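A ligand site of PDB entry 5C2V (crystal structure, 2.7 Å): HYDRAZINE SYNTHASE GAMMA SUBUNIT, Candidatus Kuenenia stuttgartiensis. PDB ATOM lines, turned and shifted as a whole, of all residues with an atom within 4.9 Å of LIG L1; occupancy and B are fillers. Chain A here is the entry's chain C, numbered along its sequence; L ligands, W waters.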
ATOM      1  N   ASN A  90      -3.606 -28.775   0.799  1.00  0.00           N
ATOM      2  CA  ASN A  90      -4.367 -28.119  -0.254  1.00  0.00           C
ATOM      3  C   ASN A  90      -4.163 -26.599  -0.189  1.00  0.00           C
ATOM      4  O   ASN A  90      -4.113 -26.019   0.889  1.00  0.00           O
ATOM      5  CB  ASN A  90      -5.853 -28.527  -0.077  1.00  0.00           C
ATOM      6  CG  ASN A  90      -6.860 -27.541  -0.646  1.00  0.00           C
ATOM      7  OD1 ASN A  90      -6.559 -26.736  -1.520  1.00  0.00           O
ATOM      8  ND2 ASN A  90      -8.080 -27.606  -0.137  1.00  0.00           N
ATOM      9  N   HIS A 105      -4.742 -24.149   8.178  1.00  0.00           N
ATOM     10  CA  HIS A 105      -5.635 -25.298   8.245  1.00  0.00           C
ATOM     11  C   HIS A 105      -5.657 -25.892   9.649  1.00  0.00           C
ATOM     12  O   HIS A 105      -6.699 -25.921  10.303  1.00  0.00           O
ATOM     13  CB  HIS A 105      -5.229 -26.376   7.229  1.00  0.00           C
ATOM     14  CG  HIS A 105      -5.801 -26.163   5.865  1.00  0.00           C
ATOM     15  ND1 HIS A 105      -5.083 -25.583   4.841  1.00  0.00           N
ATOM     16  CD2 HIS A 105      -7.009 -26.457   5.350  1.00  0.00           C
ATOM     17  CE1 HIS A 105      -5.829 -25.528   3.750  1.00  0.00           C
ATOM     18  NE2 HIS A 105      -7.008 -26.051   4.036  1.00  0.00           N
ATOM     19  N   PHE A 179     -29.226 -30.245   4.862  1.00  0.00           N
ATOM     20  CA  PHE A 179     -28.128 -29.528   5.489  1.00  0.00           C
ATOM     21  C   PHE A 179     -28.469 -29.100   6.918  1.00  0.00           C
ATOM     22  O   PHE A 179     -27.665 -29.262   7.835  1.00  0.00           O
ATOM     23  CB  PHE A 179     -27.767 -28.295   4.646  1.00  0.00           C
ATOM     24  CG  PHE A 179     -26.581 -27.525   5.165  1.00  0.00           C
ATOM     25  CD1 PHE A 179     -25.291 -27.852   4.753  1.00  0.00           C
ATOM     26  CD2 PHE A 179     -26.743 -26.464   6.042  1.00  0.00           C
ATOM     27  CE1 PHE A 179     -24.199 -27.147   5.223  1.00  0.00           C
ATOM     28  CE2 PHE A 179     -25.651 -25.758   6.511  1.00  0.00           C
ATOM     29  CZ  PHE A 179     -24.383 -26.095   6.098  1.00  0.00           C
ATOM     30  N   VAL A 184     -28.496 -34.698  10.763  1.00  0.00           N
ATOM     31  CA  VAL A 184     -27.295 -34.547   9.939  1.00  0.00           C
ATOM     32  C   VAL A 184     -26.304 -33.641  10.660  1.00  0.00           C
ATOM     33  O   VAL A 184     -25.133 -33.985  10.810  1.00  0.00           O
ATOM     34  CB  VAL A 184     -27.627 -33.980   8.553  1.00  0.00           C
ATOM     35  CG1 VAL A 184     -26.366 -33.853   7.712  1.00  0.00           C
ATOM     36  CG2 VAL A 184     -28.650 -34.863   7.844  1.00  0.00           C
ATOM     37  N   GLY A 185     -26.790 -32.475  11.082  1.00  0.00           N
ATOM     38  CA  GLY A 185     -26.030 -31.593  11.945  1.00  0.00           C
ATOM     39  C   GLY A 185     -24.908 -30.808  11.292  1.00  0.00           C
ATOM     40  O   GLY A 185     -23.834 -30.674  11.867  1.00  0.00           O
ATOM     41  N   CYS A 186     -25.161 -30.266  10.104  1.00  0.00           N
ATOM     42  CA  CYS A 186     -24.163 -29.439   9.437  1.00  0.00           C
ATOM     43  C   CYS A 186     -24.083 -28.056  10.068  1.00  0.00           C
ATOM     44  O   CYS A 186     -23.020 -27.426  10.087  1.00  0.00           O
ATOM     45  CB  CYS A 186     -24.478 -29.314   7.940  1.00  0.00           C
ATOM     46  SG  CYS A 186     -24.490 -30.870   7.032  1.00  0.00           S
ATOM     47  N   GLU A 188     -24.071 -27.221  13.050  1.00  0.00           N
ATOM     48  CA  GLU A 188     -23.289 -27.195  14.283  1.00  0.00           C
ATOM     49  C   GLU A 188     -21.941 -26.515  14.069  1.00  0.00           C
ATOM     50  O   GLU A 188     -21.623 -25.537  14.740  1.00  0.00           O
ATOM     51  CB  GLU A 188     -23.117 -28.607  14.827  1.00  0.00           C
ATOM     52  CG  GLU A 188     -24.412 -29.417  14.857  1.00  0.00           C
ATOM     53  CD  GLU A 188     -24.260 -30.770  15.522  1.00  0.00           C
ATOM     54  OE1 GLU A 188     -24.873 -30.971  16.601  1.00  0.00           O
ATOM     55  OE2 GLU A 188     -23.535 -31.625  14.988  1.00  0.00           O
ATOM     56  N   CYS A 189     -21.142 -27.045  13.145  1.00  0.00           N
ATOM     57  CA  CYS A 189     -19.859 -26.440  12.818  1.00  0.00           C
ATOM     58  C   CYS A 189     -19.914 -25.468  11.628  1.00  0.00           C
ATOM     59  O   CYS A 189     -18.953 -24.741  11.385  1.00  0.00           O
ATOM     60  CB  CYS A 189     -18.822 -27.519  12.545  1.00  0.00           C
ATOM     61  SG  CYS A 189     -18.619 -28.726  13.880  1.00  0.00           S
ATOM     62  N   HIS A 190     -21.025 -25.461  10.910  1.00  0.00           N
ATOM     63  CA  HIS A 190     -21.174 -24.584   9.747  1.00  0.00           C
ATOM     64  C   HIS A 190     -22.443 -23.731   9.811  1.00  0.00           C
ATOM     65  O   HIS A 190     -23.330 -23.870   8.962  1.00  0.00           O
ATOM     66  CB  HIS A 190     -21.176 -25.398   8.449  1.00  0.00           C
ATOM     67  CG  HIS A 190     -19.874 -26.074   8.149  1.00  0.00           C
ATOM     68  ND1 HIS A 190     -18.742 -25.381   7.770  1.00  0.00           N
ATOM     69  CD2 HIS A 190     -19.525 -27.378   8.142  1.00  0.00           C
ATOM     70  CE1 HIS A 190     -17.758 -26.228   7.557  1.00  0.00           C
ATOM     71  NE2 HIS A 190     -18.209 -27.447   7.776  1.00  0.00           N
ATOM     72  N   HIS A 207     -11.976 -28.724  15.149  1.00  0.00           N
ATOM     73  CA  HIS A 207     -12.753 -29.949  15.339  1.00  0.00           C
ATOM     74  C   HIS A 207     -12.035 -31.193  14.839  1.00  0.00           C
ATOM     75  O   HIS A 207     -11.151 -31.119  13.980  1.00  0.00           O
ATOM     76  CB  HIS A 207     -14.107 -29.831  14.639  1.00  0.00           C
ATOM     77  CG  HIS A 207     -15.018 -28.819  15.244  1.00  0.00           C
ATOM     78  ND1 HIS A 207     -15.687 -29.033  16.432  1.00  0.00           N
ATOM     79  CD2 HIS A 207     -15.391 -27.586  14.827  1.00  0.00           C
ATOM     80  CE1 HIS A 207     -16.417 -27.980  16.728  1.00  0.00           C
ATOM     81  NE2 HIS A 207     -16.268 -27.082  15.766  1.00  0.00           N
ATOM     82  N   ASP A 208     -12.421 -32.348  15.378  1.00  0.00           N
ATOM     83  CA  ASP A 208     -11.961 -33.622  14.837  1.00  0.00           C
ATOM     84  C   ASP A 208     -13.094 -34.225  14.012  1.00  0.00           C
ATOM     85  O   ASP A 208     -14.066 -34.748  14.550  1.00  0.00           O
ATOM     86  CB  ASP A 208     -11.553 -34.570  15.974  1.00  0.00           C
ATOM     87  CG  ASP A 208     -10.873 -35.843  15.478  1.00  0.00           C
ATOM     88  OD1 ASP A 208     -11.143 -36.273  14.341  1.00  0.00           O
ATOM     89  OD2 ASP A 208     -10.066 -36.411  16.247  1.00  0.00           O
ATOM     90  N   VAL A 209     -12.948 -34.158  12.690  1.00  0.00           N
ATOM     91  CA  VAL A 209     -13.926 -34.700  11.763  1.00  0.00           C
ATOM     92  C   VAL A 209     -13.519 -36.066  11.203  1.00  0.00           C
ATOM     93  O   VAL A 209     -14.188 -36.608  10.331  1.00  0.00           O
ATOM     94  CB  VAL A 209     -14.192 -33.738  10.607  1.00  0.00           C
ATOM     95  CG1 VAL A 209     -15.139 -32.636  11.054  1.00  0.00           C
ATOM     96  CG2 VAL A 209     -12.890 -33.149  10.102  1.00  0.00           C
ATOM     97  N   THR A 211     -10.687 -36.608   9.598  1.00  0.00           N
ATOM     98  CA  THR A 211      -9.933 -36.392   8.368  1.00  0.00           C
ATOM     99  C   THR A 211      -8.429 -36.440   8.601  1.00  0.00           C
ATOM    100  O   THR A 211      -7.648 -36.262   7.670  1.00  0.00           O
ATOM    101  CB  THR A 211     -10.289 -35.040   7.727  1.00  0.00           C
ATOM    102  OG1 THR A 211     -10.094 -33.987   8.678  1.00  0.00           O
ATOM    103  CG2 THR A 211     -11.737 -35.037   7.261  1.00  0.00           C
ATOM    104  N   PHE A 256      -8.545 -29.834  12.882  1.00  0.00           N
ATOM    105  CA  PHE A 256      -8.334 -28.731  11.950  1.00  0.00           C
ATOM    106  C   PHE A 256      -9.335 -27.589  12.104  1.00  0.00           C
ATOM    107  O   PHE A 256     -10.466 -27.791  12.524  1.00  0.00           O
ATOM    108  CB  PHE A 256      -8.371 -29.252  10.510  1.00  0.00           C
ATOM    109  CG  PHE A 256      -7.520 -30.470  10.283  1.00  0.00           C
ATOM    110  CD1 PHE A 256      -6.158 -30.339  10.048  1.00  0.00           C
ATOM    111  CD2 PHE A 256      -8.073 -31.734  10.312  1.00  0.00           C
ATOM    112  CE1 PHE A 256      -5.367 -31.461   9.851  1.00  0.00           C
ATOM    113  CE2 PHE A 256      -7.292 -32.857  10.109  1.00  0.00           C
ATOM    114  CZ  PHE A 256      -5.934 -32.714   9.881  1.00  0.00           C
ATOM    115  N   ASP A 257      -8.900 -26.390  11.745  1.00  0.00           N
ATOM    116  CA  ASP A 257      -9.747 -25.207  11.727  1.00  0.00           C
ATOM    117  C   ASP A 257     -10.760 -25.294  10.584  1.00  0.00           C
ATOM    118  O   ASP A 257     -10.384 -25.511   9.433  1.00  0.00           O
ATOM    119  CB  ASP A 257      -8.901 -23.943  11.611  1.00  0.00           C
ATOM    120  CG  ASP A 257      -9.712 -22.710  11.249  1.00  0.00           C
ATOM    121  OD1 ASP A 257     -10.476 -22.231  12.107  1.00  0.00           O
ATOM    122  OD2 ASP A 257      -9.566 -22.221  10.111  1.00  0.00           O
ATOM    123  N   THR A 258     -12.038 -25.132  10.899  1.00  0.00           N
ATOM    124  CA  THR A 258     -13.099 -25.266   9.913  1.00  0.00           C
ATOM    125  C   THR A 258     -13.128 -24.105   8.925  1.00  0.00           C
ATOM    126  O   THR A 258     -13.189 -22.942   9.333  1.00  0.00           O
ATOM    127  CB  THR A 258     -14.484 -25.385  10.576  1.00  0.00           C
ATOM    128  OG1 THR A 258     -14.984 -24.072  10.893  1.00  0.00           O
ATOM    129  CG2 THR A 258     -14.408 -26.227  11.830  1.00  0.00           C
ATOM    130  N   PRO A 259     -13.079 -24.415   7.626  1.00  0.00           N
ATOM    131  CA  PRO A 259     -13.154 -23.428   6.541  1.00  0.00           C
ATOM    132  C   PRO A 259     -14.587 -22.951   6.284  1.00  0.00           C
ATOM    133  O   PRO A 259     -15.534 -23.640   6.650  1.00  0.00           O
ATOM    134  CB  PRO A 259     -12.620 -24.194   5.328  1.00  0.00           C
ATOM    135  CG  PRO A 259     -12.098 -25.507   5.854  1.00  0.00           C
ATOM    136  CD  PRO A 259     -12.851 -25.770   7.104  1.00  0.00           C
ATOM    137  N   THR A 260     -14.713 -21.795   5.654  1.00  0.00           N
ATOM    138  CA  THR A 260     -16.024 -21.306   5.222  1.00  0.00           C
ATOM    139  C   THR A 260     -16.588 -22.207   4.128  1.00  0.00           C
ATOM    140  O   THR A 260     -15.835 -22.859   3.399  1.00  0.00           O
ATOM    141  CB  THR A 260     -15.945 -19.859   4.690  1.00  0.00           C
ATOM    142  OG1 THR A 260     -17.250 -19.439   4.273  1.00  0.00           O
ATOM    143  CG2 THR A 260     -14.992 -19.772   3.513  1.00  0.00           C
ATOM    144  N   LEU A 261     -17.910 -22.266   4.030  1.00  0.00           N
ATOM    145  CA  LEU A 261     -18.544 -22.993   2.935  1.00  0.00           C
ATOM    146  C   LEU A 261     -18.920 -22.035   1.804  1.00  0.00           C
ATOM    147  O   LEU A 261     -19.450 -22.462   0.775  1.00  0.00           O
ATOM    148  CB  LEU A 261     -19.779 -23.748   3.426  1.00  0.00           C
ATOM    149  CG  LEU A 261     -19.511 -24.839   4.460  1.00  0.00           C
ATOM    150  CD1 LEU A 261     -20.734 -25.728   4.645  1.00  0.00           C
ATOM    151  CD2 LEU A 261     -18.288 -25.666   4.074  1.00  0.00           C
ATOM    152  N   ILE A 264     -17.548 -22.441  -2.001  1.00  0.00           N
ATOM    153  CA  ILE A 264     -16.988 -23.780  -1.926  1.00  0.00           C
ATOM    154  C   ILE A 264     -17.056 -24.462  -3.301  1.00  0.00           C
ATOM    155  O   ILE A 264     -16.427 -25.483  -3.534  1.00  0.00           O
ATOM    156  CB  ILE A 264     -17.712 -24.650  -0.883  1.00  0.00           C
ATOM    157  CG1 ILE A 264     -16.837 -25.823  -0.441  1.00  0.00           C
ATOM    158  CG2 ILE A 264     -19.051 -25.145  -1.414  1.00  0.00           C
ATOM    159  CD1 ILE A 264     -15.545 -25.398   0.227  1.00  0.00           C
ATOM    160  N   SER A 267     -13.456 -23.956  -4.784  1.00  0.00           N
ATOM    161  CA  SER A 267     -12.260 -24.583  -4.212  1.00  0.00           C
ATOM    162  C   SER A 267     -12.034 -25.895  -4.922  1.00  0.00           C
ATOM    163  O   SER A 267     -12.845 -26.811  -4.840  1.00  0.00           O
ATOM    164  CB  SER A 267     -12.411 -24.825  -2.697  1.00  0.00           C
ATOM    165  OG  SER A 267     -11.541 -25.865  -2.243  1.00  0.00           O
ATOM    166  N   TYR A 270     -11.382 -30.309  -1.912  1.00  0.00           N
ATOM    167  CA  TYR A 270     -11.631 -29.968  -0.507  1.00  0.00           C
ATOM    168  C   TYR A 270     -10.904 -30.768   0.597  1.00  0.00           C
ATOM    169  O   TYR A 270     -10.068 -31.627   0.338  1.00  0.00           O
ATOM    170  CB  TYR A 270     -13.134 -30.072  -0.258  1.00  0.00           C
ATOM    171  CG  TYR A 270     -13.905 -29.567  -1.449  1.00  0.00           C
ATOM    172  CD1 TYR A 270     -14.046 -28.209  -1.664  1.00  0.00           C
ATOM    173  CD2 TYR A 270     -14.427 -30.446  -2.388  1.00  0.00           C
ATOM    174  CE1 TYR A 270     -14.725 -27.742  -2.754  1.00  0.00           C
ATOM    175  CE2 TYR A 270     -15.104 -29.982  -3.500  1.00  0.00           C
ATOM    176  CZ  TYR A 270     -15.249 -28.618  -3.671  1.00  0.00           C
ATOM    177  OH  TYR A 270     -15.922 -28.132  -4.772  1.00  0.00           O
ATOM    178  N   PHE A 271     -11.315 -30.467   1.832  1.00  0.00           N
ATOM    179  CA  PHE A 271     -10.622 -30.664   3.115  1.00  0.00           C
ATOM    180  C   PHE A 271      -9.228 -30.024   3.189  1.00  0.00           C
ATOM    181  O   PHE A 271      -8.956 -29.063   2.476  1.00  0.00           O
ATOM    182  CB  PHE A 271     -10.512 -32.168   3.430  1.00  0.00           C
ATOM    183  CG  PHE A 271     -11.820 -32.804   3.819  1.00  0.00           C
ATOM    184  CD1 PHE A 271     -12.780 -32.081   4.511  1.00  0.00           C
ATOM    185  CD2 PHE A 271     -12.084 -34.118   3.490  1.00  0.00           C
ATOM    186  CE1 PHE A 271     -13.985 -32.654   4.861  1.00  0.00           C
ATOM    187  CE2 PHE A 271     -13.289 -34.701   3.840  1.00  0.00           C
ATOM    188  CZ  PHE A 271     -14.235 -33.969   4.528  1.00  0.00           C
ATOM    189  N   HIS A 272      -8.353 -30.563   4.033  1.00  0.00           N
ATOM    190  CA  HIS A 272      -7.043 -29.929   4.259  1.00  0.00           C
ATOM    191  C   HIS A 272      -5.932 -30.408   3.323  1.00  0.00           C
ATOM    192  O   HIS A 272      -5.145 -29.603   2.823  1.00  0.00           O
ATOM    193  CB  HIS A 272      -6.612 -30.083   5.727  1.00  0.00           C
ATOM    194  CG  HIS A 272      -6.216 -31.471   6.123  1.00  0.00           C
ATOM    195  ND1 HIS A 272      -7.117 -32.508   6.190  1.00  0.00           N
ATOM    196  CD2 HIS A 272      -5.015 -31.977   6.487  1.00  0.00           C
ATOM    197  CE1 HIS A 272      -6.488 -33.601   6.581  1.00  0.00           C
ATOM    198  NE2 HIS A 272      -5.209 -33.317   6.760  1.00  0.00           N
ATOM    199  N   LEU A 279     -17.241 -32.442  -4.070  1.00  0.00           N
ATOM    200  CA  LEU A 279     -18.073 -32.072  -2.925  1.00  0.00           C
ATOM    201  C   LEU A 279     -18.724 -33.310  -2.316  1.00  0.00           C
ATOM    202  O   LEU A 279     -18.794 -33.454  -1.088  1.00  0.00           O
ATOM    203  CB  LEU A 279     -19.141 -31.062  -3.345  1.00  0.00           C
ATOM    204  CG  LEU A 279     -18.670 -29.641  -3.633  1.00  0.00           C
ATOM    205  CD1 LEU A 279     -19.718 -28.864  -4.398  1.00  0.00           C
ATOM    206  CD2 LEU A 279     -18.339 -28.934  -2.321  1.00  0.00           C
ATOM    207  N   THR A 282     -17.002 -35.193   0.433  1.00  0.00           N
ATOM    208  CA  THR A 282     -16.934 -34.599   1.762  1.00  0.00           C
ATOM    209  C   THR A 282     -18.081 -35.109   2.630  1.00  0.00           C
ATOM    210  O   THR A 282     -18.228 -34.734   3.796  1.00  0.00           O
ATOM    211  CB  THR A 282     -16.995 -33.059   1.701  1.00  0.00           C
ATOM    212  OG1 THR A 282     -18.230 -32.647   1.101  1.00  0.00           O
ATOM    213  CG2 THR A 282     -15.840 -32.511   0.891  1.00  0.00           C
ATOM    214  N   ILE A 283     -18.883 -35.981   2.039  1.00  0.00           N
ATOM    215  CA  ILE A 283     -20.169 -36.404   2.575  1.00  0.00           C
ATOM    216  C   ILE A 283     -20.240 -37.927   2.656  1.00  0.00           C
ATOM    217  O   ILE A 283     -20.481 -38.505   3.711  1.00  0.00           O
ATOM    218  CB  ILE A 283     -21.337 -35.855   1.745  1.00  0.00           C
ATOM    219  CG1 ILE A 283     -21.308 -34.326   1.768  1.00  0.00           C
ATOM    220  CG2 ILE A 283     -22.650 -36.359   2.277  1.00  0.00           C
ATOM    221  CD1 ILE A 283     -22.364 -33.685   0.899  1.00  0.00           C
ATOM    222  N   MET A 292     -18.093 -39.039  11.162  1.00  0.00           N
ATOM    223  CA  MET A 292     -17.278 -38.111  11.933  1.00  0.00           C
ATOM    224  C   MET A 292     -17.389 -36.694  11.367  1.00  0.00           C
ATOM    225  O   MET A 292     -17.151 -35.709  12.069  1.00  0.00           O
ATOM    226  CB  MET A 292     -15.831 -38.568  11.980  1.00  0.00           C
ATOM    227  CG  MET A 292     -15.572 -39.675  12.974  1.00  0.00           C
ATOM    228  SD  MET A 292     -15.869 -39.147  14.679  1.00  0.00           S
ATOM    229  CE  MET A 292     -15.595 -40.685  15.562  1.00  0.00           C
ATOM    230  N   HIS A 293     -17.747 -36.606  10.090  1.00  0.00           N
ATOM    231  CA  HIS A 293     -18.113 -35.328   9.490  1.00  0.00           C
ATOM    232  C   HIS A 293     -19.577 -35.419   9.077  1.00  0.00           C
ATOM    233  O   HIS A 293     -19.900 -35.995   8.038  1.00  0.00           O
ATOM    234  CB  HIS A 293     -17.200 -35.030   8.301  1.00  0.00           C
ATOM    235  CG  HIS A 293     -17.343 -33.653   7.733  1.00  0.00           C
ATOM    236  ND1 HIS A 293     -17.736 -33.427   6.422  1.00  0.00           N
ATOM    237  CD2 HIS A 293     -17.134 -32.439   8.271  1.00  0.00           C
ATOM    238  CE1 HIS A 293     -17.760 -32.125   6.196  1.00  0.00           C
ATOM    239  NE2 HIS A 293     -17.406 -31.501   7.295  1.00  0.00           N
ATOM    240  N   GLY A 294     -20.456 -34.824   9.879  1.00  0.00           N
ATOM    241  CA  GLY A 294     -21.898 -34.979   9.719  1.00  0.00           C
ATOM    242  C   GLY A 294     -22.322 -36.424   9.992  1.00  0.00           C
ATOM    243  O   GLY A 294     -21.465 -37.310  10.040  1.00  0.00           O
ATOM    244  N   THR A 296     -24.120 -38.798   7.777  1.00  0.00           N
ATOM    245  CA  THR A 296     -24.692 -38.984   6.454  1.00  0.00           C
ATOM    246  C   THR A 296     -25.011 -40.435   6.076  1.00  0.00           C
ATOM    247  O   THR A 296     -25.528 -40.689   4.991  1.00  0.00           O
ATOM    248  CB  THR A 296     -23.763 -38.384   5.395  1.00  0.00           C
ATOM    249  OG1 THR A 296     -22.451 -38.958   5.517  1.00  0.00           O
ATOM    250  CG2 THR A 296     -23.656 -36.879   5.616  1.00  0.00           C
ATOM    251  N   LEU A 307     -27.878 -32.202  -1.421  1.00  0.00           N
ATOM    252  CA  LEU A 307     -26.983 -31.553  -0.468  1.00  0.00           C
ATOM    253  C   LEU A 307     -25.778 -30.943  -1.195  1.00  0.00           C
ATOM    254  O   LEU A 307     -25.345 -29.836  -0.868  1.00  0.00           O
ATOM    255  CB  LEU A 307     -26.517 -32.556   0.583  1.00  0.00           C
ATOM    256  CG  LEU A 307     -25.639 -32.021   1.723  1.00  0.00           C
ATOM    257  CD1 LEU A 307     -26.260 -30.773   2.333  1.00  0.00           C
ATOM    258  CD2 LEU A 307     -25.445 -33.096   2.780  1.00  0.00           C
ATOM    259  N   LEU A 311     -24.659 -27.061  -1.464  1.00  0.00           N
ATOM    260  CA  LEU A 311     -23.285 -26.629  -1.225  1.00  0.00           C
ATOM    261  C   LEU A 311     -22.796 -25.759  -2.384  1.00  0.00           C
ATOM    262  O   LEU A 311     -22.105 -24.757  -2.173  1.00  0.00           O
ATOM    263  CB  LEU A 311     -22.366 -27.840  -1.037  1.00  0.00           C
ATOM    264  CG  LEU A 311     -22.525 -28.595   0.281  1.00  0.00           C
ATOM    265  CD1 LEU A 311     -21.697 -29.873   0.265  1.00  0.00           C
ATOM    266  CD2 LEU A 311     -22.112 -27.710   1.448  1.00  0.00           C
HETATM  267 FE1  LIG L   1     -17.758 -29.558   7.522  1.00  0.00          FE
HETATM  268  C1  LIG L   1     -14.743 -29.017   5.967  1.00  0.00           C
HETATM  269  C2  LIG L   1     -19.358 -29.406   4.495  1.00  0.00           C
HETATM  270  C3  LIG L   1     -20.621 -30.817   8.966  1.00  0.00           C
HETATM  271  C4  LIG L   1     -16.293 -29.366  10.596  1.00  0.00           C
HETATM  272  N1  LIG L   1     -17.161 -29.289   5.581  1.00  0.00           N
HETATM  273  C5  LIG L   1     -15.867 -29.032   5.161  1.00  0.00           C
HETATM  274  C6  LIG L   1     -15.906 -28.772   3.737  1.00  0.00           C
HETATM  275  C7  LIG L   1     -17.173 -28.876   3.333  1.00  0.00           C
HETATM  276  C8  LIG L   1     -17.987 -29.213   4.483  1.00  0.00           C
HETATM  277  C9  LIG L   1     -17.686 -28.688   1.879  1.00  0.00           C
HETATM  278  C10 LIG L   1     -14.695 -28.429   2.840  1.00  0.00           C
HETATM  279  C11 LIG L   1     -14.168 -27.048   3.196  1.00  0.00           C
HETATM  280  C12 LIG L   1     -12.854 -26.800   2.502  1.00  0.00           C
HETATM  281  O1  LIG L   1     -12.412 -25.627   2.452  1.00  0.00           O
HETATM  282  O2  LIG L   1     -12.253 -27.780   1.991  1.00  0.00           O
HETATM  283  N2  LIG L   1     -19.668 -29.954   6.871  1.00  0.00           N
HETATM  284  C13 LIG L   1     -20.057 -29.964   5.541  1.00  0.00           C
HETATM  285  C14 LIG L   1     -21.328 -30.660   5.447  1.00  0.00           C
HETATM  286  C15 LIG L   1     -21.685 -31.047   6.684  1.00  0.00           C
HETATM  287  C16 LIG L   1     -20.643 -30.610   7.597  1.00  0.00           C
HETATM  288  C17 LIG L   1     -22.117 -30.889   4.134  1.00  0.00           C
HETATM  289  C18 LIG L   1     -22.956 -31.824   7.084  1.00  0.00           C
HETATM  290  C19 LIG L   1     -22.874 -33.284   6.581  1.00  0.00           C
HETATM  291  N3  LIG L   1     -18.344 -30.005   9.426  1.00  0.00           N
HETATM  292  C20 LIG L   1     -19.574 -30.522   9.809  1.00  0.00           C
HETATM  293  C21 LIG L   1     -19.508 -30.803  11.230  1.00  0.00           C
HETATM  294  C22 LIG L   1     -18.364 -30.293  11.693  1.00  0.00           C
HETATM  295  C23 LIG L   1     -17.576 -29.852  10.556  1.00  0.00           C
HETATM  296  C24 LIG L   1     -20.716 -31.231  12.094  1.00  0.00           C
HETATM  297  C25 LIG L   1     -17.886 -30.285  13.164  1.00  0.00           C
HETATM  298  C26 LIG L   1     -17.624 -31.726  13.664  1.00  0.00           C
HETATM  299  N4  LIG L   1     -15.809 -29.172   8.187  1.00  0.00           N
HETATM  300  C27 LIG L   1     -15.435 -29.303   9.518  1.00  0.00           C
HETATM  301  C28 LIG L   1     -13.990 -29.373   9.584  1.00  0.00           C
HETATM  302  C29 LIG L   1     -13.501 -29.254   8.127  1.00  0.00           C
HETATM  303  C30 LIG L   1     -14.710 -29.144   7.330  1.00  0.00           C
HETATM  304  C31 LIG L   1     -13.115 -29.516  10.856  1.00  0.00           C
HETATM  305  C32 LIG L   1     -12.056 -29.277   7.609  1.00  0.00           C
HETATM  306  C33 LIG L   1     -11.446 -30.653   7.854  1.00  0.00           C
HETATM  307  C34 LIG L   1     -10.162 -30.788   7.095  1.00  0.00           C
HETATM  308  O3  LIG L   1      -9.550 -31.890   7.140  1.00  0.00           O
HETATM  309  O4  LIG L   1      -9.747 -29.803   6.434  1.00  0.00           O
HETATM  310  N1  LG2 L   2     -16.601 -34.024  18.791  1.00  0.00           N
HETATM  311  C1  LG2 L   2     -15.727 -33.634  17.598  1.00  0.00           C
HETATM  312  C2  LG2 L   2     -14.956 -32.227  17.903  1.00  0.00           C
HETATM  313  O1  LG2 L   2     -15.685 -31.210  17.808  1.00  0.00           O
HETATM  314  O2  LG2 L   2     -13.737 -32.371  18.184  1.00  0.00           O
HETATM  315  C3  LG2 L   2     -15.901 -33.702  20.103  1.00  0.00           C
HETATM  316  C4  LG2 L   2     -16.869 -35.536  18.768  1.00  0.00           C
HETATM  317  C5  LG2 L   2     -17.899 -33.253  18.777  1.00  0.00           C
HETATM  318  O   HOH W   1     -13.042 -22.779   2.316  1.00  0.00           O
HETATM  319  O   HOH W   2      -9.156 -27.394   7.408  1.00  0.00           O
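C18 of LIG L1 is covalently linked to SG of Cys 186 (1.8 Å).
C25 of LIG L1 is covalently linked to SG of Cys 189, at 1.9 Å.
NE2 of His 293 is bound to FE1 of LIG L1.
A ring nitrogen (NE2) of His 190 is bound to an iron atom (FE1) of LIG L1, 2.2 Å away.
O3 of LIG L1 lies within hydrogen-bond range of OG1 of Thr 211.
An oxygen (O4) of LIG L1 lies within hydrogen-bond range of the backbone NH of His 272, at 2.9 Å.
O3 of LIG L1 lies within hydrogen-bond range of ND1 of His 272 (2.7 Å).
An oxygen (O2) of LIG L1 is in hydrogen-bond range of the backbone NH (N) of Phe 271 (2.9 Å).
ND1 of His 207 lies within hydrogen-bond range of O1 of LG2 L2 (2.6 Å).
An oxygen (O2) of LG2 L2 lies within hydrogen-bond range of the backbone NH of Asp 208 (3.1 Å).
NE2 of His 207 sits at hydrogen-bond distance from SG of Cys 189 (3.4 Å).
A ring nitrogen (ND1) of His 293 lies within hydrogen-bond range of the backbone carbonyl oxygen of Thr 282, 3.0 Å away.
The backbone carbonyl oxygen of His 272 sits at hydrogen-bond distance from the backbone NH of Asn 90, at 2.7 Å.
The backbone carbonyl oxygen of Phe 271 sits close to the side-chain amide nitrogen of Asn 90 (3.1 Å).
OH of Tyr 270 sits close to O of Ile 264, 3.0 Å away.
The side-chain hydroxyl of Tyr 270 lies close to the backbone carbonyl oxygen of Ser 267 (3.3 Å).
The backbone NH (N) of Phe 256 is in hydrogen-bond range of the backbone carbonyl oxygen (O) of His 207, at 3.1 Å.
The backbone carbonyl oxygen (O) of Ile 283 sits at hydrogen-bond distance from the side-chain hydroxyl (OG1) of Thr 296.
CG1 of Val 184 touches C19 of LIG L1, at 3.7 Å.
Gly 185 touches LIG L1.
His 207 touches LIG L1 (CG to C25, 3.8 Å).
Val 209 touches LIG L1 (CG1 to C4, 3.5 Å).
Phe 256 touches LIG L1.
Thr 258 touches LIG L1 (CG2 to C31, 3.7 Å).
Pro 259 touches LIG L1 (CB to O1, 3.2 Å).
Leu 261 touches LIG L1.
Ile 264 touches LIG L1.
Tyr 270 touches LIG L1 (CB to O2, 3.3 Å).
CA of Gly 294 touches C19 of LIG L1 (3.7 Å).
CG2 of Thr 296 touches C19 of LIG L1 (3.8 Å).
Hydrophobic or aromatic side chains that line LIG L1: Val 184, His 190, His 207, Val 209, Phe 256, Pro 259, Leu 261, Ile 264, Tyr 270, Phe 271, His 272 and His 293.
Within 4 Å of LIG L1: Val 184, Gly 185, Cys 186, Cys 189, His 190, His 207, Val 209, Thr 211, Phe 256, Thr 258, Pro 259, Leu 261, Ile 264, Tyr 270, Phe 271, His 272, His 293, Gly 294 and Thr 296.
The nearest printed residue that does not touch LIG L1 is Leu 311 (4.02 Å).
Water W2 bridges O4 of LIG L1 (2.7 Å) and O of Asp 257 (3.0 Å).
Water W1 lies within hydrogen-bond range of an oxygen (O1) of LIG L1 (2.9 Å) and the backbone carbonyl oxygen of Thr 260 (3.0 Å).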
